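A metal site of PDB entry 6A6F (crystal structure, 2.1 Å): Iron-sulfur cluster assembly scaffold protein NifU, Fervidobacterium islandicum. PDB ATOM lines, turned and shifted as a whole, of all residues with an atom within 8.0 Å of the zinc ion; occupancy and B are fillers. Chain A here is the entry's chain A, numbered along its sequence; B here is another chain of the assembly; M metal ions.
O of Asp 39 lies within hydrogen-bond range of N of Asn 34 (2.9 Å). O of Cys 62 sits at hydrogen-bond distance from OG of Ser 65 (3.1 Å). The backbone NH (N) of Ile 64 lies close to the side-chain sulfur (SG) of Cys 62 (3.6 Å). OD1 of Asn 34 sits at hydrogen-bond distance from OG of Ser 36 (3.0 Å). OD1 of Asp 39 lies within hydrogen-bond range of OG of Ser 65 (3.4 Å). The side-chain sulfur (SG) of Cys 123 lies close to the side-chain amide nitrogen (ND2) of Asn 34 (3.4 Å). The side-chain sulfur (SG) of Cys 123 lies close to the guanidinium group (NE) of Arg 120, 3.5 Å away. The side-chain sulfur (SG) of Cys 62 lies close to the guanidinium group (NH1) of Arg 120 (3.2 Å).
The zinc ion is bound by OD2 of Asp 39 (2.1 Å), SG of Cys 62 (2.3 Å), SG of Cys 123 (2.3 Å) and SG of Cys 37 (2.4 Å). The zinc ion has four donor atoms within binding distance.
Asn 34 touches the zinc ion (ND2 to ZN, 3.99 Å). Five residues have an atom within 4 Å of the zinc ion: Asn 34, Cys 37, Asp 39, Cys 62 and Cys 123.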
ATOM      1  N   TYR A   6       4.886  -6.063  -1.791  1.00  0.00           N
ATOM      2  CA  TYR A   6       4.331  -4.782  -1.339  1.00  0.00           C
ATOM      3  C   TYR A   6       3.312  -4.910  -0.216  1.00  0.00           C
ATOM      4  O   TYR A   6       2.123  -4.872  -0.484  1.00  0.00           O
ATOM      5  CB  TYR A   6       3.693  -4.035  -2.531  1.00  0.00           C
ATOM      6  CG  TYR A   6       4.723  -3.682  -3.611  1.00  0.00           C
ATOM      7  CD1 TYR A   6       5.737  -2.755  -3.365  1.00  0.00           C
ATOM      8  CD2 TYR A   6       4.697  -4.297  -4.841  1.00  0.00           C
ATOM      9  CE1 TYR A   6       6.670  -2.442  -4.326  1.00  0.00           C
ATOM     10  CE2 TYR A   6       5.621  -3.991  -5.838  1.00  0.00           C
ATOM     11  CZ  TYR A   6       6.594  -3.064  -5.585  1.00  0.00           C
ATOM     12  OH  TYR A   6       7.511  -2.792  -6.557  1.00  0.00           O
ATOM     13  N   ASN A  34      20.259   4.126  -7.026  1.00  0.00           N
ATOM     14  CA  ASN A  34      20.228   2.671  -7.296  1.00  0.00           C
ATOM     15  C   ASN A  34      19.786   2.601  -8.736  1.00  0.00           C
ATOM     16  O   ASN A  34      18.579   2.555  -9.043  1.00  0.00           O
ATOM     17  CB  ASN A  34      19.217   1.942  -6.375  1.00  0.00           C
ATOM     18  CG  ASN A  34      18.928   0.497  -6.802  1.00  0.00           C
ATOM     19  OD1 ASN A  34      19.817  -0.203  -7.268  1.00  0.00           O
ATOM     20  ND2 ASN A  34      17.696   0.049  -6.583  1.00  0.00           N
ATOM     21  N   SER A  36      19.985   0.340 -11.089  1.00  0.00           N
ATOM     22  CA  SER A  36      19.299  -0.843 -11.623  1.00  0.00           C
ATOM     23  C   SER A  36      17.787  -0.715 -11.536  1.00  0.00           C
ATOM     24  O   SER A  36      17.129  -1.403 -12.299  1.00  0.00           O
ATOM     25  CB  SER A  36      19.786  -2.144 -10.954  1.00  0.00           C
ATOM     26  OG  SER A  36      19.512  -2.200  -9.549  1.00  0.00           O
ATOM     27  N   CYS A  37      17.266   0.159 -10.648  1.00  0.00           N
ATOM     28  CA  CYS A  37      15.830   0.427 -10.501  1.00  0.00           C
ATOM     29  C   CYS A  37      15.403   1.846 -10.906  1.00  0.00           C
ATOM     30  O   CYS A  37      14.277   2.032 -11.393  1.00  0.00           O
ATOM     31  CB  CYS A  37      15.343   0.131  -9.026  1.00  0.00           C
ATOM     32  SG  CYS A  37      13.555   0.341  -8.725  1.00  0.00           S
ATOM     33  N   GLY A  38      16.282   2.843 -10.713  1.00  0.00           N
ATOM     34  CA  GLY A  38      15.949   4.252 -10.969  1.00  0.00           C
ATOM     35  C   GLY A  38      15.663   5.071  -9.702  1.00  0.00           C
ATOM     36  O   GLY A  38      15.071   6.174  -9.782  1.00  0.00           O
ATOM     37  N   ASP A  39      16.096   4.572  -8.543  1.00  0.00           N
ATOM     38  CA  ASP A  39      15.842   5.211  -7.238  1.00  0.00           C
ATOM     39  C   ASP A  39      16.902   6.265  -6.951  1.00  0.00           C
ATOM     40  O   ASP A  39      18.090   6.041  -7.208  1.00  0.00           O
ATOM     41  CB  ASP A  39      15.851   4.169  -6.110  1.00  0.00           C
ATOM     42  CG  ASP A  39      14.864   3.066  -6.345  1.00  0.00           C
ATOM     43  OD1 ASP A  39      13.746   3.363  -6.786  1.00  0.00           O
ATOM     44  OD2 ASP A  39      15.197   1.909  -6.041  1.00  0.00           O
ATOM     45  N   GLU A  40      16.460   7.412  -6.439  1.00  0.00           N
ATOM     46  CA  GLU A  40      17.376   8.506  -6.040  1.00  0.00           C
ATOM     47  C   GLU A  40      16.988   8.968  -4.661  1.00  0.00           C
ATOM     48  O   GLU A  40      15.826   9.077  -4.376  1.00  0.00           O
ATOM     49  CB  GLU A  40      17.242   9.701  -6.961  1.00  0.00           C
ATOM     50  CG  GLU A  40      17.839   9.412  -8.334  1.00  0.00           C
ATOM     51  CD  GLU A  40      17.707  10.605  -9.278  1.00  0.00           C
ATOM     52  OE1 GLU A  40      18.252  10.494 -10.401  1.00  0.00           O
ATOM     53  OE2 GLU A  40      17.098  11.649  -8.892  1.00  0.00           O
ATOM     54  N   HIS A  60      13.162  10.700  -5.342  1.00  0.00           N
ATOM     55  CA  HIS A  60      12.070   9.774  -5.327  1.00  0.00           C
ATOM     56  C   HIS A  60      12.522   8.469  -5.903  1.00  0.00           C
ATOM     57  O   HIS A  60      13.586   8.370  -6.503  1.00  0.00           O
ATOM     58  CB  HIS A  60      10.854  10.330  -6.079  1.00  0.00           C
ATOM     59  CG  HIS A  60      11.031  10.341  -7.562  1.00  0.00           C
ATOM     60  ND1 HIS A  60      11.802  11.290  -8.201  1.00  0.00           N
ATOM     61  CD2 HIS A  60      10.598   9.494  -8.534  1.00  0.00           C
ATOM     62  CE1 HIS A  60      11.806  11.052  -9.498  1.00  0.00           C
ATOM     63  NE2 HIS A  60      11.089   9.968  -9.727  1.00  0.00           N
ATOM     64  N   GLY A  61      11.683   7.479  -5.731  1.00  0.00           N
ATOM     65  CA  GLY A  61      11.992   6.140  -6.186  1.00  0.00           C
ATOM     66  C   GLY A  61      10.811   5.196  -5.999  1.00  0.00           C
ATOM     67  O   GLY A  61       9.696   5.607  -5.716  1.00  0.00           O
ATOM     68  N   CYS A  62      11.082   3.904  -6.127  1.00  0.00           N
ATOM     69  CA  CYS A  62      10.074   2.908  -5.869  1.00  0.00           C
ATOM     70  C   CYS A  62       9.503   2.937  -4.413  1.00  0.00           C
ATOM     71  O   CYS A  62      10.004   3.638  -3.498  1.00  0.00           O
ATOM     72  CB  CYS A  62      10.653   1.546  -6.215  1.00  0.00           C
ATOM     73  SG  CYS A  62      11.805   0.789  -5.055  1.00  0.00           S
ATOM     74  N   ALA A  63       8.457   2.158  -4.200  1.00  0.00           N
ATOM     75  CA  ALA A  63       7.840   2.070  -2.908  1.00  0.00           C
ATOM     76  C   ALA A  63       8.745   1.474  -1.818  1.00  0.00           C
ATOM     77  O   ALA A  63       8.637   1.865  -0.644  1.00  0.00           O
ATOM     78  CB  ALA A  63       6.522   1.282  -3.013  1.00  0.00           C
ATOM     79  N   ILE A  64       9.598   0.550  -2.183  1.00  0.00           N
ATOM     80  CA  ILE A  64      10.489  -0.093  -1.265  1.00  0.00           C
ATOM     81  C   ILE A  64      11.606   0.875  -0.819  1.00  0.00           C
ATOM     82  O   ILE A  64      11.863   0.962   0.408  1.00  0.00           O
ATOM     83  CB  ILE A  64      11.087  -1.379  -1.849  1.00  0.00           C
ATOM     84  CG1 ILE A  64      10.014  -2.461  -2.000  1.00  0.00           C
ATOM     85  CG2 ILE A  64      12.194  -1.903  -0.956  1.00  0.00           C
ATOM     86  CD1 ILE A  64      10.514  -3.703  -2.727  1.00  0.00           C
ATOM     87  N   SER A  65      12.228   1.580  -1.771  1.00  0.00           N
ATOM     88  CA  SER A  65      13.240   2.584  -1.432  1.00  0.00           C
ATOM     89  C   SER A  65      12.671   3.757  -0.596  1.00  0.00           C
ATOM     90  O   SER A  65      13.316   4.185   0.351  1.00  0.00           O
ATOM     91  CB  SER A  65      13.992   3.144  -2.663  1.00  0.00           C
ATOM     92  OG  SER A  65      13.095   3.928  -3.484  1.00  0.00           O
ATOM     93  N   GLN A  66      11.478   4.253  -0.948  1.00  0.00           N
ATOM     94  CA  GLN A  66      10.817   5.345  -0.217  1.00  0.00           C
ATOM     95  C   GLN A  66      10.327   4.889   1.166  1.00  0.00           C
ATOM     96  O   GLN A  66      10.545   5.630   2.159  1.00  0.00           O
ATOM     97  CB  GLN A  66       9.660   6.013  -0.998  1.00  0.00           C
ATOM     98  CG  GLN A  66      10.064   6.696  -2.286  1.00  0.00           C
ATOM     99  CD  GLN A  66       8.972   7.546  -2.982  1.00  0.00           C
ATOM    100  OE1 GLN A  66       9.296   8.279  -3.892  1.00  0.00           O
ATOM    101  NE2 GLN A  66       7.704   7.478  -2.541  1.00  0.00           N
ATOM    102  N   MET A 119      17.101  -8.189  -6.473  1.00  0.00           N
ATOM    103  CA  MET A 119      17.110  -6.861  -7.092  1.00  0.00           C
ATOM    104  C   MET A 119      16.561  -5.766  -6.142  1.00  0.00           C
ATOM    105  O   MET A 119      17.156  -4.672  -6.050  1.00  0.00           O
ATOM    106  CB  MET A 119      16.413  -6.847  -8.452  1.00  0.00           C
ATOM    107  CG  MET A 119      17.400  -7.023  -9.612  1.00  0.00           C
ATOM    108  SD  MET A 119      16.586  -6.858 -11.218  1.00  0.00           S
ATOM    109  CE  MET A 119      15.642  -8.386 -11.334  1.00  0.00           C
ATOM    110  N   ARG A 120      15.507  -6.101  -5.396  1.00  0.00           N
ATOM    111  CA  ARG A 120      14.882  -5.160  -4.464  1.00  0.00           C
ATOM    112  C   ARG A 120      15.675  -4.927  -3.168  1.00  0.00           C
ATOM    113  O   ARG A 120      15.454  -3.955  -2.461  1.00  0.00           O
ATOM    114  CB  ARG A 120      13.443  -5.574  -4.145  1.00  0.00           C
ATOM    115  CG  ARG A 120      12.612  -5.926  -5.367  1.00  0.00           C
ATOM    116  CD  ARG A 120      12.741  -4.886  -6.498  1.00  0.00           C
ATOM    117  NE  ARG A 120      12.211  -3.590  -6.114  1.00  0.00           N
ATOM    118  CZ  ARG A 120      10.947  -3.231  -6.185  1.00  0.00           C
ATOM    119  NH1 ARG A 120      10.599  -2.027  -5.789  1.00  0.00           N
ATOM    120  NH2 ARG A 120      10.013  -4.086  -6.607  1.00  0.00           N
ATOM    121  N   VAL A 121      16.603  -5.799  -2.868  1.00  0.00           N
ATOM    122  CA  VAL A 121      17.512  -5.592  -1.770  1.00  0.00           C
ATOM    123  C   VAL A 121      18.267  -4.277  -1.903  1.00  0.00           C
ATOM    124  O   VAL A 121      18.545  -3.616  -0.920  1.00  0.00           O
ATOM    125  CB  VAL A 121      18.511  -6.765  -1.656  1.00  0.00           C
ATOM    126  CG1 VAL A 121      19.659  -6.422  -0.723  1.00  0.00           C
ATOM    127  CG2 VAL A 121      17.796  -7.982  -1.129  1.00  0.00           C
ATOM    128  N   LYS A 122      18.606  -3.905  -3.122  1.00  0.00           N
ATOM    129  CA  LYS A 122      19.262  -2.634  -3.369  1.00  0.00           C
ATOM    130  C   LYS A 122      18.388  -1.410  -3.104  1.00  0.00           C
ATOM    131  O   LYS A 122      18.915  -0.384  -2.750  1.00  0.00           O
ATOM    132  CB  LYS A 122      19.741  -2.564  -4.814  1.00  0.00           C
ATOM    133  CG  LYS A 122      21.058  -3.293  -5.009  1.00  0.00           C
ATOM    134  CD  LYS A 122      20.881  -4.644  -5.681  1.00  0.00           C
ATOM    135  CE  LYS A 122      21.933  -4.813  -6.770  1.00  0.00           C
ATOM    136  NZ  LYS A 122      21.733  -3.680  -7.691  1.00  0.00           N
ATOM    137  N   CYS A 123      17.082  -1.540  -3.342  1.00  0.00           N
ATOM    138  CA  CYS A 123      16.086  -0.537  -3.049  1.00  0.00           C
ATOM    139  C   CYS A 123      15.967  -0.317  -1.531  1.00  0.00           C
ATOM    140  O   CYS A 123      16.041   0.802  -1.076  1.00  0.00           O
ATOM    141  CB  CYS A 123      14.721  -0.919  -3.653  1.00  0.00           C
ATOM    142  SG  CYS A 123      14.804  -1.398  -5.418  1.00  0.00           S
ATOM    143  N   PHE A 124      15.801  -1.400  -0.771  1.00  0.00           N
ATOM    144  CA  PHE A 124      15.845  -1.328   0.658  1.00  0.00           C
ATOM    145  C   PHE A 124      17.115  -0.683   1.220  1.00  0.00           C
ATOM    146  O   PHE A 124      17.049   0.142   2.152  1.00  0.00           O
ATOM    147  CB  PHE A 124      15.761  -2.721   1.265  1.00  0.00           C
ATOM    148  CG  PHE A 124      15.928  -2.707   2.736  1.00  0.00           C
ATOM    149  CD1 PHE A 124      14.971  -2.145   3.554  1.00  0.00           C
ATOM    150  CD2 PHE A 124      17.063  -3.223   3.320  1.00  0.00           C
ATOM    151  CE1 PHE A 124      15.122  -2.131   4.948  1.00  0.00           C
ATOM    152  CE2 PHE A 124      17.236  -3.203   4.696  1.00  0.00           C
ATOM    153  CZ  PHE A 124      16.271  -2.648   5.514  1.00  0.00           C
ATOM    154  N   LEU A 126      19.353   1.313  -0.265  1.00  0.00           N
ATOM    155  CA  LEU A 126      19.793   2.590  -0.778  1.00  0.00           C
ATOM    156  C   LEU A 126      19.897   3.692   0.330  1.00  0.00           C
ATOM    157  O   LEU A 126      20.949   4.283   0.499  1.00  0.00           O
ATOM    158  CB  LEU A 126      18.877   3.065  -1.923  1.00  0.00           C
ATOM    159  CG  LEU A 126      19.189   4.480  -2.435  1.00  0.00           C
ATOM    160  CD1 LEU A 126      20.607   4.517  -2.965  1.00  0.00           C
ATOM    161  CD2 LEU A 126      18.204   4.913  -3.495  1.00  0.00           C
ATOM    162  N   LYS B  15       6.637   1.883 -11.497  1.00  0.00           N
ATOM    163  CA  LYS B  15       8.079   1.845 -11.572  1.00  0.00           C
ATOM    164  C   LYS B  15       8.668   2.076 -12.988  1.00  0.00           C
ATOM    165  O   LYS B  15       9.873   2.278 -13.105  1.00  0.00           O
ATOM    166  CB  LYS B  15       8.572   0.459 -11.143  1.00  0.00           C
ATOM    167  CG  LYS B  15       8.357   0.149  -9.703  1.00  0.00           C
ATOM    168  CD  LYS B  15       9.265  -1.038  -9.314  1.00  0.00           C
ATOM    169  CE  LYS B  15       8.792  -2.348  -9.890  1.00  0.00           C
ATOM    170  NZ  LYS B  15       7.370  -2.573  -9.499  1.00  0.00           N
HETATM  171 ZN    ZN M   1      13.744   0.484  -6.306  1.00  0.00          ZN
